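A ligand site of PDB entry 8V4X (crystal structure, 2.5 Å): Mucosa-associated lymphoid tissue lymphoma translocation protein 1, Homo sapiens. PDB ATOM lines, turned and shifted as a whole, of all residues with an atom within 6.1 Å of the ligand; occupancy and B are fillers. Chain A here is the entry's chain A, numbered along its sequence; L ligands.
The side-chain amide nitrogen (ND2) of Asn 61 is in hydrogen-bond range of a nitrogen (N4) of the ligand (2.9 Å). A nitrogen (N7) of the ligand lies within hydrogen-bond range of the side-chain carboxylate (OE1) of Glu 65 (2.9 Å).
The backbone NH (N) of Ala 13 sits at hydrogen-bond distance from the backbone carbonyl oxygen (O) of Lys 47. The side-chain amide oxygen (OE1) of Gln 344 is in hydrogen-bond range of the side-chain amide nitrogen (ND2) of Asn 278 (2.9 Å). The backbone carbonyl oxygen (O) of Trp 248 sits at hydrogen-bond distance from a ring nitrogen (ND1) of His 252 (2.9 Å). The backbone carbonyl oxygen (O) of Leu 69 sits at hydrogen-bond distance from the guanidinium group (NE) of Arg 244. The side-chain amide nitrogen (ND2) of Asn 61 lies close to the side-chain hydroxyl (OH) of Tyr 57 (3.4 Å). The side-chain carboxylate of Glu 58 lies within salt-bridge range of the side-chain amino group of Lys 345 (3.4 Å). The side-chain amide nitrogen of Gln 344 is in hydrogen-bond range of the side-chain carboxylate of Glu 58 (2.7 Å). The backbone NH of Lys 47 is in hydrogen-bond range of the backbone carbonyl oxygen of Lys 11.
The backbone carbonyl oxygen (O) of Ala 13 lies close to a sulfur (S1) of the ligand, 3.5 Å away. The backbone carbonyl oxygen (O) of Glu 58 lies close to a fluorine (F3) of the ligand, 2.9 Å away. Merely in contact with the ligand: Trp 248 (3.2 Å), Gln 344 (3.2 Å), Met 385 (3.3 Å), Lys 47 (3.3 Å), Leu 69 (3.3 Å), Leu 51 (3.4 Å), Ala 62 (3.5 Å), Ala 251 (3.5 Å), Leu 14 (3.6 Å), Leu 54 (3.6 Å), Tyr 57 (3.7 Å), Ile 380 (3.7 Å), Val 49 (3.7 Å), Gln 247 (3.7 Å), Leu 383 (3.7 Å), Val 12 (3.7 Å) and Phe 66 (3.7 Å). Hydrophobic or aromatic side chains within 4 Å of the ligand: Val 12, Leu 14, Val 49, Leu 51, Leu 54, Tyr 57, Ala 62, Phe 66, Leu 69, Trp 248, Ala 251, Ile 380, Leu 383 and Met 385. Along chain A the residues within 4 Å of the ligand span positions 12 to 385.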
ATOM      1  N   LYS A  11       0.793  -4.576  22.760  1.00  0.00           N
ATOM      2  CA  LYS A  11       0.950  -5.731  21.868  1.00  0.00           C
ATOM      3  C   LYS A  11       0.948  -5.193  20.444  1.00  0.00           C
ATOM      4  O   LYS A  11      -0.121  -4.860  19.917  1.00  0.00           O
ATOM      5  CB  LYS A  11      -0.184  -6.757  22.074  1.00  0.00           C
ATOM      6  CG  LYS A  11      -0.113  -7.475  23.416  1.00  0.00           C
ATOM      7  CD  LYS A  11      -0.947  -8.755  23.470  1.00  0.00           C
ATOM      8  CE  LYS A  11      -2.411  -8.419  23.479  1.00  0.00           C
ATOM      9  NZ  LYS A  11      -3.245  -9.631  23.668  1.00  0.00           N
ATOM     10  N   VAL A  12       2.140  -5.038  19.829  1.00  0.00           N
ATOM     11  CA  VAL A  12       2.215  -4.488  18.482  1.00  0.00           C
ATOM     12  C   VAL A  12       2.787  -5.488  17.456  1.00  0.00           C
ATOM     13  O   VAL A  12       3.655  -6.281  17.803  1.00  0.00           O
ATOM     14  CB  VAL A  12       2.961  -3.128  18.452  1.00  0.00           C
ATOM     15  CG1 VAL A  12       2.200  -2.081  19.240  1.00  0.00           C
ATOM     16  CG2 VAL A  12       4.373  -3.275  18.988  1.00  0.00           C
ATOM     17  N   ALA A  13       2.308  -5.417  16.203  1.00  0.00           N
ATOM     18  CA  ALA A  13       2.787  -6.338  15.186  1.00  0.00           C
ATOM     19  C   ALA A  13       2.997  -5.755  13.778  1.00  0.00           C
ATOM     20  O   ALA A  13       2.132  -5.062  13.267  1.00  0.00           O
ATOM     21  CB  ALA A  13       1.848  -7.541  15.116  1.00  0.00           C
ATOM     22  N   LEU A  14       4.114  -6.094  13.125  1.00  0.00           N
ATOM     23  CA  LEU A  14       4.384  -5.652  11.759  1.00  0.00           C
ATOM     24  C   LEU A  14       4.276  -6.881  10.868  1.00  0.00           C
ATOM     25  O   LEU A  14       4.903  -7.895  11.148  1.00  0.00           O
ATOM     26  CB  LEU A  14       5.786  -5.016  11.610  1.00  0.00           C
ATOM     27  CG  LEU A  14       6.323  -4.800  10.186  1.00  0.00           C
ATOM     28  CD1 LEU A  14       5.675  -3.632   9.533  1.00  0.00           C
ATOM     29  CD2 LEU A  14       7.827  -4.643  10.192  1.00  0.00           C
ATOM     30  N   LYS A  47      -2.022  -4.240  17.744  1.00  0.00           N
ATOM     31  CA  LYS A  47      -2.177  -3.112  16.824  1.00  0.00           C
ATOM     32  C   LYS A  47      -1.352  -3.535  15.638  1.00  0.00           C
ATOM     33  O   LYS A  47      -0.131  -3.630  15.763  1.00  0.00           O
ATOM     34  CB  LYS A  47      -1.626  -1.808  17.418  1.00  0.00           C
ATOM     35  CG  LYS A  47      -2.586  -1.055  18.317  1.00  0.00           C
ATOM     36  CD  LYS A  47      -1.834  -0.050  19.189  1.00  0.00           C
ATOM     37  CE  LYS A  47      -2.247  -0.150  20.641  1.00  0.00           C
ATOM     38  NZ  LYS A  47      -2.260  -1.572  21.128  1.00  0.00           N
ATOM     39  N   VAL A  48      -1.966  -3.852  14.520  1.00  0.00           N
ATOM     40  CA  VAL A  48      -1.257  -4.364  13.356  1.00  0.00           C
ATOM     41  C   VAL A  48      -1.091  -3.343  12.222  1.00  0.00           C
ATOM     42  O   VAL A  48      -2.002  -2.576  11.925  1.00  0.00           O
ATOM     43  CB  VAL A  48      -1.951  -5.646  12.806  1.00  0.00           C
ATOM     44  CG1 VAL A  48      -1.103  -6.326  11.743  1.00  0.00           C
ATOM     45  CG2 VAL A  48      -2.271  -6.638  13.926  1.00  0.00           C
ATOM     46  N   VAL A  49       0.071  -3.367  11.593  1.00  0.00           N
ATOM     47  CA  VAL A  49       0.377  -2.661  10.354  1.00  0.00           C
ATOM     48  C   VAL A  49       0.695  -3.834   9.404  1.00  0.00           C
ATOM     49  O   VAL A  49       1.498  -4.732   9.736  1.00  0.00           O
ATOM     50  CB  VAL A  49       1.505  -1.584  10.490  1.00  0.00           C
ATOM     51  CG1 VAL A  49       2.534  -1.649   9.358  1.00  0.00           C
ATOM     52  CG2 VAL A  49       0.901  -0.188  10.577  1.00  0.00           C
ATOM     53  N   LEU A  51       1.604  -4.670   5.450  1.00  0.00           N
ATOM     54  CA  LEU A  51       2.059  -4.151   4.174  1.00  0.00           C
ATOM     55  C   LEU A  51       2.262  -5.205   3.087  1.00  0.00           C
ATOM     56  O   LEU A  51       2.751  -6.298   3.347  1.00  0.00           O
ATOM     57  CB  LEU A  51       3.344  -3.325   4.377  1.00  0.00           C
ATOM     58  CG  LEU A  51       3.154  -2.142   5.304  1.00  0.00           C
ATOM     59  CD1 LEU A  51       4.448  -1.731   5.955  1.00  0.00           C
ATOM     60  CD2 LEU A  51       2.445  -1.010   4.627  1.00  0.00           C
ATOM     61  N   LEU A  54       6.639  -4.787  -0.630  1.00  0.00           N
ATOM     62  CA  LEU A  54       7.522  -3.683  -0.311  1.00  0.00           C
ATOM     63  C   LEU A  54       8.886  -3.894  -0.953  1.00  0.00           C
ATOM     64  O   LEU A  54       9.388  -5.009  -1.024  1.00  0.00           O
ATOM     65  CB  LEU A  54       7.680  -3.471   1.198  1.00  0.00           C
ATOM     66  CG  LEU A  54       6.445  -3.344   2.029  1.00  0.00           C
ATOM     67  CD1 LEU A  54       6.809  -3.249   3.456  1.00  0.00           C
ATOM     68  CD2 LEU A  54       5.614  -2.168   1.629  1.00  0.00           C
ATOM     69  N   TYR A  57      13.865  -0.366   0.311  1.00  0.00           N
ATOM     70  CA  TYR A  57      13.771   0.894   1.057  1.00  0.00           C
ATOM     71  C   TYR A  57      12.569   0.903   1.993  1.00  0.00           C
ATOM     72  O   TYR A  57      12.696   1.280   3.157  1.00  0.00           O
ATOM     73  CB  TYR A  57      13.725   2.096   0.102  1.00  0.00           C
ATOM     74  CG  TYR A  57      13.603   3.445   0.800  1.00  0.00           C
ATOM     75  CD1 TYR A  57      14.517   3.849   1.754  1.00  0.00           C
ATOM     76  CD2 TYR A  57      12.579   4.328   0.464  1.00  0.00           C
ATOM     77  CE1 TYR A  57      14.415   5.081   2.389  1.00  0.00           C
ATOM     78  CE2 TYR A  57      12.459   5.561   1.099  1.00  0.00           C
ATOM     79  CZ  TYR A  57      13.378   5.945   2.060  1.00  0.00           C
ATOM     80  OH  TYR A  57      13.247   7.169   2.675  1.00  0.00           O
ATOM     81  N   GLU A  58      11.401   0.459   1.484  1.00  0.00           N
ATOM     82  CA  GLU A  58      10.141   0.416   2.206  1.00  0.00           C
ATOM     83  C   GLU A  58      10.142  -0.625   3.335  1.00  0.00           C
ATOM     84  O   GLU A  58       9.492  -0.422   4.348  1.00  0.00           O
ATOM     85  CB  GLU A  58       9.011   0.153   1.236  1.00  0.00           C
ATOM     86  CG  GLU A  58       9.029   1.123   0.071  1.00  0.00           C
ATOM     87  CD  GLU A  58       8.010   0.901  -1.025  1.00  0.00           C
ATOM     88  OE1 GLU A  58       7.453  -0.215  -1.104  1.00  0.00           O
ATOM     89  OE2 GLU A  58       7.786   1.850  -1.814  1.00  0.00           O
ATOM     90  N   MET A  59      10.887  -1.727   3.159  1.00  0.00           N
ATOM     91  CA  MET A  59      10.987  -2.744   4.193  1.00  0.00           C
ATOM     92  C   MET A  59      11.881  -2.235   5.336  1.00  0.00           C
ATOM     93  O   MET A  59      11.581  -2.427   6.514  1.00  0.00           O
ATOM     94  CB  MET A  59      11.588  -4.037   3.620  1.00  0.00           C
ATOM     95  CG  MET A  59      10.694  -4.745   2.647  1.00  0.00           C
ATOM     96  SD  MET A  59      11.152  -6.474   2.395  1.00  0.00           S
ATOM     97  CE  MET A  59      10.948  -7.103   4.060  1.00  0.00           C
ATOM     98  N   ASN A  61      12.381   0.937   6.096  1.00  0.00           N
ATOM     99  CA  ASN A  61      11.684   2.002   6.839  1.00  0.00           C
ATOM    100  C   ASN A  61      10.625   1.483   7.795  1.00  0.00           C
ATOM    101  O   ASN A  61      10.485   2.027   8.893  1.00  0.00           O
ATOM    102  CB  ASN A  61      11.070   3.015   5.892  1.00  0.00           C
ATOM    103  CG  ASN A  61      12.060   4.007   5.346  1.00  0.00           C
ATOM    104  OD1 ASN A  61      13.225   4.074   5.759  1.00  0.00           O
ATOM    105  ND2 ASN A  61      11.592   4.794   4.393  1.00  0.00           N
ATOM    106  N   ALA A  62       9.863   0.453   7.388  1.00  0.00           N
ATOM    107  CA  ALA A  62       8.827  -0.143   8.213  1.00  0.00           C
ATOM    108  C   ALA A  62       9.436  -0.920   9.373  1.00  0.00           C
ATOM    109  O   ALA A  62       8.915  -0.871  10.478  1.00  0.00           O
ATOM    110  CB  ALA A  62       7.954  -1.056   7.377  1.00  0.00           C
ATOM    111  N   VAL A  63      10.542  -1.649   9.123  1.00  0.00           N
ATOM    112  CA  VAL A  63      11.202  -2.423  10.171  1.00  0.00           C
ATOM    113  C   VAL A  63      11.726  -1.490  11.253  1.00  0.00           C
ATOM    114  O   VAL A  63      11.437  -1.691  12.428  1.00  0.00           O
ATOM    115  CB  VAL A  63      12.278  -3.397   9.611  1.00  0.00           C
ATOM    116  CG1 VAL A  63      13.394  -3.685  10.618  1.00  0.00           C
ATOM    117  CG2 VAL A  63      11.641  -4.702   9.130  1.00  0.00           C
ATOM    118  N   GLU A  65      10.837   1.676  12.011  1.00  0.00           N
ATOM    119  CA  GLU A  65       9.788   2.334  12.792  1.00  0.00           C
ATOM    120  C   GLU A  65       9.054   1.405  13.737  1.00  0.00           C
ATOM    121  O   GLU A  65       8.531   1.863  14.745  1.00  0.00           O
ATOM    122  CB  GLU A  65       8.809   3.085  11.896  1.00  0.00           C
ATOM    123  CG  GLU A  65       9.464   4.278  11.243  1.00  0.00           C
ATOM    124  CD  GLU A  65       8.563   5.151  10.393  1.00  0.00           C
ATOM    125  OE1 GLU A  65       7.327   5.002  10.473  1.00  0.00           O
ATOM    126  OE2 GLU A  65       9.112   5.980   9.632  1.00  0.00           O
ATOM    127  N   PHE A  66       9.014   0.093  13.412  1.00  0.00           N
ATOM    128  CA  PHE A  66       8.389  -0.919  14.263  1.00  0.00           C
ATOM    129  C   PHE A  66       9.238  -1.090  15.543  1.00  0.00           C
ATOM    130  O   PHE A  66       8.703  -1.155  16.647  1.00  0.00           O
ATOM    131  CB  PHE A  66       8.276  -2.234  13.482  1.00  0.00           C
ATOM    132  CG  PHE A  66       7.919  -3.473  14.276  1.00  0.00           C
ATOM    133  CD1 PHE A  66       6.636  -3.668  14.750  1.00  0.00           C
ATOM    134  CD2 PHE A  66       8.854  -4.465  14.495  1.00  0.00           C
ATOM    135  CE1 PHE A  66       6.303  -4.805  15.456  1.00  0.00           C
ATOM    136  CE2 PHE A  66       8.526  -5.609  15.207  1.00  0.00           C
ATOM    137  CZ  PHE A  66       7.257  -5.776  15.684  1.00  0.00           C
ATOM    138  N   LEU A  69       8.769   1.681  18.061  1.00  0.00           N
ATOM    139  CA  LEU A  69       7.542   1.515  18.839  1.00  0.00           C
ATOM    140  C   LEU A  69       7.664   0.480  19.966  1.00  0.00           C
ATOM    141  O   LEU A  69       6.906   0.542  20.941  1.00  0.00           O
ATOM    142  CB  LEU A  69       6.337   1.168  17.956  1.00  0.00           C
ATOM    143  CG  LEU A  69       5.680   2.304  17.167  1.00  0.00           C
ATOM    144  CD1 LEU A  69       4.289   1.898  16.730  1.00  0.00           C
ATOM    145  CD2 LEU A  69       5.584   3.603  17.990  1.00  0.00           C
ATOM    146  N   ARG A 244       2.611   6.106  20.887  1.00  0.00           N
ATOM    147  CA  ARG A 244       2.620   4.899  20.062  1.00  0.00           C
ATOM    148  C   ARG A 244       1.266   4.800  19.363  1.00  0.00           C
ATOM    149  O   ARG A 244       1.200   4.556  18.156  1.00  0.00           O
ATOM    150  CB  ARG A 244       2.858   3.637  20.927  1.00  0.00           C
ATOM    151  CG  ARG A 244       2.780   2.319  20.146  1.00  0.00           C
ATOM    152  CD  ARG A 244       2.933   1.086  21.022  1.00  0.00           C
ATOM    153  NE  ARG A 244       4.220   1.046  21.722  1.00  0.00           N
ATOM    154  CZ  ARG A 244       4.367   1.199  23.038  1.00  0.00           C
ATOM    155  NH1 ARG A 244       3.315   1.384  23.814  1.00  0.00           N
ATOM    156  NH2 ARG A 244       5.579   1.172  23.574  1.00  0.00           N
ATOM    157  N   GLN A 247       0.904   7.750  16.617  1.00  0.00           N
ATOM    158  CA  GLN A 247       1.613   7.499  15.370  1.00  0.00           C
ATOM    159  C   GLN A 247       0.991   6.359  14.574  1.00  0.00           C
ATOM    160  O   GLN A 247       0.995   6.386  13.344  1.00  0.00           O
ATOM    161  CB  GLN A 247       3.092   7.186  15.662  1.00  0.00           C
ATOM    162  CG  GLN A 247       4.008   7.660  14.553  1.00  0.00           C
ATOM    163  CD  GLN A 247       4.035   9.160  14.505  1.00  0.00           C
ATOM    164  OE1 GLN A 247       3.625   9.774  13.511  1.00  0.00           O
ATOM    165  NE2 GLN A 247       4.497   9.788  15.574  1.00  0.00           N
ATOM    166  N   TRP A 248       0.464   5.356  15.271  1.00  0.00           N
ATOM    167  CA  TRP A 248      -0.181   4.204  14.647  1.00  0.00           C
ATOM    168  C   TRP A 248      -1.558   4.597  14.091  1.00  0.00           C
ATOM    169  O   TRP A 248      -1.975   4.030  13.080  1.00  0.00           O
ATOM    170  CB  TRP A 248      -0.264   3.044  15.640  1.00  0.00           C
ATOM    171  CG  TRP A 248      -1.166   1.921  15.214  1.00  0.00           C
ATOM    172  CD1 TRP A 248      -0.828   0.854  14.431  1.00  0.00           C
ATOM    173  CD2 TRP A 248      -2.545   1.778  15.538  1.00  0.00           C
ATOM    174  NE1 TRP A 248      -1.927   0.048  14.255  1.00  0.00           N
ATOM    175  CE2 TRP A 248      -2.995   0.598  14.906  1.00  0.00           C
ATOM    176  CE3 TRP A 248      -3.454   2.542  16.274  1.00  0.00           C
ATOM    177  CZ2 TRP A 248      -4.320   0.170  14.998  1.00  0.00           C
ATOM    178  CZ3 TRP A 248      -4.756   2.115  16.382  1.00  0.00           C
ATOM    179  CH2 TRP A 248      -5.182   0.946  15.740  1.00  0.00           C
ATOM    180  N   ALA A 251      -1.360   6.356  10.492  1.00  0.00           N
ATOM    181  CA  ALA A 251      -1.209   5.470   9.352  1.00  0.00           C
ATOM    182  C   ALA A 251      -2.483   4.649   9.020  1.00  0.00           C
ATOM    183  O   ALA A 251      -2.421   3.782   8.146  1.00  0.00           O
ATOM    184  CB  ALA A 251      -0.044   4.532   9.560  1.00  0.00           C
ATOM    185  N   HIS A 252      -3.607   4.887   9.724  1.00  0.00           N
ATOM    186  CA  HIS A 252      -4.830   4.123   9.479  1.00  0.00           C
ATOM    187  C   HIS A 252      -6.049   5.010   9.340  1.00  0.00           C
ATOM    188  O   HIS A 252      -7.127   4.681   9.831  1.00  0.00           O
ATOM    189  CB  HIS A 252      -5.036   3.030  10.536  1.00  0.00           C
ATOM    190  CG  HIS A 252      -4.011   1.952  10.414  1.00  0.00           C
ATOM    191  ND1 HIS A 252      -2.834   1.996  11.147  1.00  0.00           N
ATOM    192  CD2 HIS A 252      -3.969   0.885   9.587  1.00  0.00           C
ATOM    193  CE1 HIS A 252      -2.140   0.928  10.771  1.00  0.00           C
ATOM    194  NE2 HIS A 252      -2.785   0.236   9.832  1.00  0.00           N
ATOM    195  N   ASN A 278      -1.346  -0.524   3.086  1.00  0.00           N
ATOM    196  CA  ASN A 278      -0.987   0.195   1.868  1.00  0.00           C
ATOM    197  C   ASN A 278      -1.947  -0.085   0.689  1.00  0.00           C
ATOM    198  O   ASN A 278      -1.651   0.305  -0.453  1.00  0.00           O
ATOM    199  CB  ASN A 278       0.464  -0.032   1.475  1.00  0.00           C
ATOM    200  CG  ASN A 278       0.834  -1.444   1.193  1.00  0.00           C
ATOM    201  OD1 ASN A 278       0.240  -2.395   1.711  1.00  0.00           O
ATOM    202  ND2 ASN A 278       1.868  -1.634   0.369  1.00  0.00           N
ATOM    203  N   GLN A 344       2.059   3.671  -0.333  1.00  0.00           N
ATOM    204  CA  GLN A 344       3.361   4.127   0.168  1.00  0.00           C
ATOM    205  C   GLN A 344       4.279   4.717  -0.922  1.00  0.00           C
ATOM    206  O   GLN A 344       5.280   5.349  -0.599  1.00  0.00           O
ATOM    207  CB  GLN A 344       4.072   3.015   0.953  1.00  0.00           C
ATOM    208  CG  GLN A 344       4.915   2.058   0.120  1.00  0.00           C
ATOM    209  CD  GLN A 344       4.142   0.989  -0.595  1.00  0.00           C
ATOM    210  OE1 GLN A 344       2.916   0.906  -0.495  1.00  0.00           O
ATOM    211  NE2 GLN A 344       4.824   0.127  -1.324  1.00  0.00           N
ATOM    212  N   LYS A 345       3.959   4.494  -2.210  1.00  0.00           N
ATOM    213  CA  LYS A 345       4.724   5.040  -3.337  1.00  0.00           C
ATOM    214  C   LYS A 345       4.231   6.425  -3.774  1.00  0.00           C
ATOM    215  O   LYS A 345       4.691   6.913  -4.795  1.00  0.00           O
ATOM    216  CB  LYS A 345       4.656   4.096  -4.545  1.00  0.00           C
ATOM    217  CG  LYS A 345       5.323   2.747  -4.350  1.00  0.00           C
ATOM    218  CD  LYS A 345       5.549   2.046  -5.680  1.00  0.00           C
ATOM    219  CE  LYS A 345       6.228   0.702  -5.552  1.00  0.00           C
ATOM    220  NZ  LYS A 345       7.644   0.808  -5.094  1.00  0.00           N
ATOM    221  N   ILE A 380      -1.160   4.460   4.870  1.00  0.00           N
ATOM    222  CA  ILE A 380       0.288   4.620   5.044  1.00  0.00           C
ATOM    223  C   ILE A 380       0.911   5.779   4.215  1.00  0.00           C
ATOM    224  O   ILE A 380       2.041   6.200   4.469  1.00  0.00           O
ATOM    225  CB  ILE A 380       1.009   3.272   4.773  1.00  0.00           C
ATOM    226  CG1 ILE A 380       2.290   3.117   5.625  1.00  0.00           C
ATOM    227  CG2 ILE A 380       1.279   3.054   3.278  1.00  0.00           C
ATOM    228  CD1 ILE A 380       2.016   2.853   7.042  1.00  0.00           C
ATOM    229  N   LEU A 383       2.725   8.867   5.788  1.00  0.00           N
ATOM    230  CA  LEU A 383       4.091   8.810   6.275  1.00  0.00           C
ATOM    231  C   LEU A 383       5.024   9.125   5.109  1.00  0.00           C
ATOM    232  O   LEU A 383       5.960   8.367   4.820  1.00  0.00           O
ATOM    233  CB  LEU A 383       4.399   7.422   6.868  1.00  0.00           C
ATOM    234  CG  LEU A 383       3.402   6.782   7.814  1.00  0.00           C
ATOM    235  CD1 LEU A 383       4.033   5.625   8.478  1.00  0.00           C
ATOM    236  CD2 LEU A 383       2.919   7.739   8.884  1.00  0.00           C
ATOM    237  N   MET A 385       7.473   9.480   2.612  1.00  0.00           N
ATOM    238  CA  MET A 385       8.885   9.166   2.465  1.00  0.00           C
ATOM    239  C   MET A 385       9.273   8.991   0.983  1.00  0.00           C
ATOM    240  O   MET A 385       8.778   8.075   0.322  1.00  0.00           O
ATOM    241  CB  MET A 385       9.238   7.899   3.239  1.00  0.00           C
ATOM    242  CG  MET A 385      10.285   8.122   4.305  1.00  0.00           C
ATOM    243  SD  MET A 385       9.523   8.403   5.915  1.00  0.00           S
ATOM    244  CE  MET A 385       9.978   6.935   6.684  1.00  0.00           C
HETATM  245  N1  LIG L   1       5.676   2.029  10.493  1.00  0.00           N
HETATM  246  N2  LIG L   1       5.004  -1.195  12.068  1.00  0.00           N
HETATM  247  C1  LIG L   1       4.105  -0.810  12.976  1.00  0.00           C
HETATM  248  C2  LIG L   1       2.451  -0.550  14.735  1.00  0.00           C
HETATM  249  C3  LIG L   1       1.491  -0.749  15.850  1.00  0.00           C
HETATM  250  C4  LIG L   1       5.485  -0.254  11.253  1.00  0.00           C
HETATM  251  C5  LIG L   1       3.648   2.873  12.541  1.00  0.00           C
HETATM  252  C6  LIG L   1       2.578   3.320  11.562  1.00  0.00           C
HETATM  253  C7  LIG L   1       7.614   3.730   4.691  1.00  0.00           C
HETATM  254  C8  LIG L   1       9.066   4.298   1.603  1.00  0.00           C
HETATM  255  C9  LIG L   1       6.660   2.212   6.275  1.00  0.00           C
HETATM  256  F1  LIG L   1       5.095   1.593   3.815  1.00  0.00           F
HETATM  257  C10 LIG L   1       6.413   1.482   3.973  1.00  0.00           C
HETATM  258  F2  LIG L   1       6.895   1.625   2.733  1.00  0.00           F
HETATM  259  F3  LIG L   1       6.683   0.225   4.343  1.00  0.00           F
HETATM  260  C11 LIG L   1       6.953   2.492   4.942  1.00  0.00           C
HETATM  261  N3  LIG L   1       7.919   4.092   3.339  1.00  0.00           N
HETATM  262  N4  LIG L   1       9.183   4.013   2.889  1.00  0.00           N
HETATM  263  C12 LIG L   1       7.728   4.557   1.307  1.00  0.00           C
HETATM  264  N5  LIG L   1       7.009   4.428   2.418  1.00  0.00           N
HETATM  265  N6  LIG L   1       7.937   4.622   5.630  1.00  0.00           N
HETATM  266  C13 LIG L   1       7.601   4.314   6.889  1.00  0.00           C
HETATM  267  C14 LIG L   1       6.962   3.141   7.267  1.00  0.00           C
HETATM  268  N7  LIG L   1       6.588   2.940   8.616  1.00  0.00           N
HETATM  269  C15 LIG L   1       5.833   1.922   9.133  1.00  0.00           C
HETATM  270  O1  LIG L   1       5.361   1.017   8.462  1.00  0.00           O
HETATM  271  C16 LIG L   1       5.084   1.071  11.345  1.00  0.00           C
HETATM  272  S1  LIG L   1       3.379  -1.892  14.126  1.00  0.00           S
HETATM  273  N8  LIG L   1       2.658   0.590  14.150  1.00  0.00           N
HETATM  274  C17 LIG L   1       3.608   0.453  13.147  1.00  0.00           C
HETATM  275  C18 LIG L   1       4.133   1.438  12.305  1.00  0.00           C
HETATM  276  O2  LIG L   1       4.707   3.807  12.409  1.00  0.00           O
HETATM  277  C19 LIG L   1       5.192   4.258  13.673  1.00  0.00           C
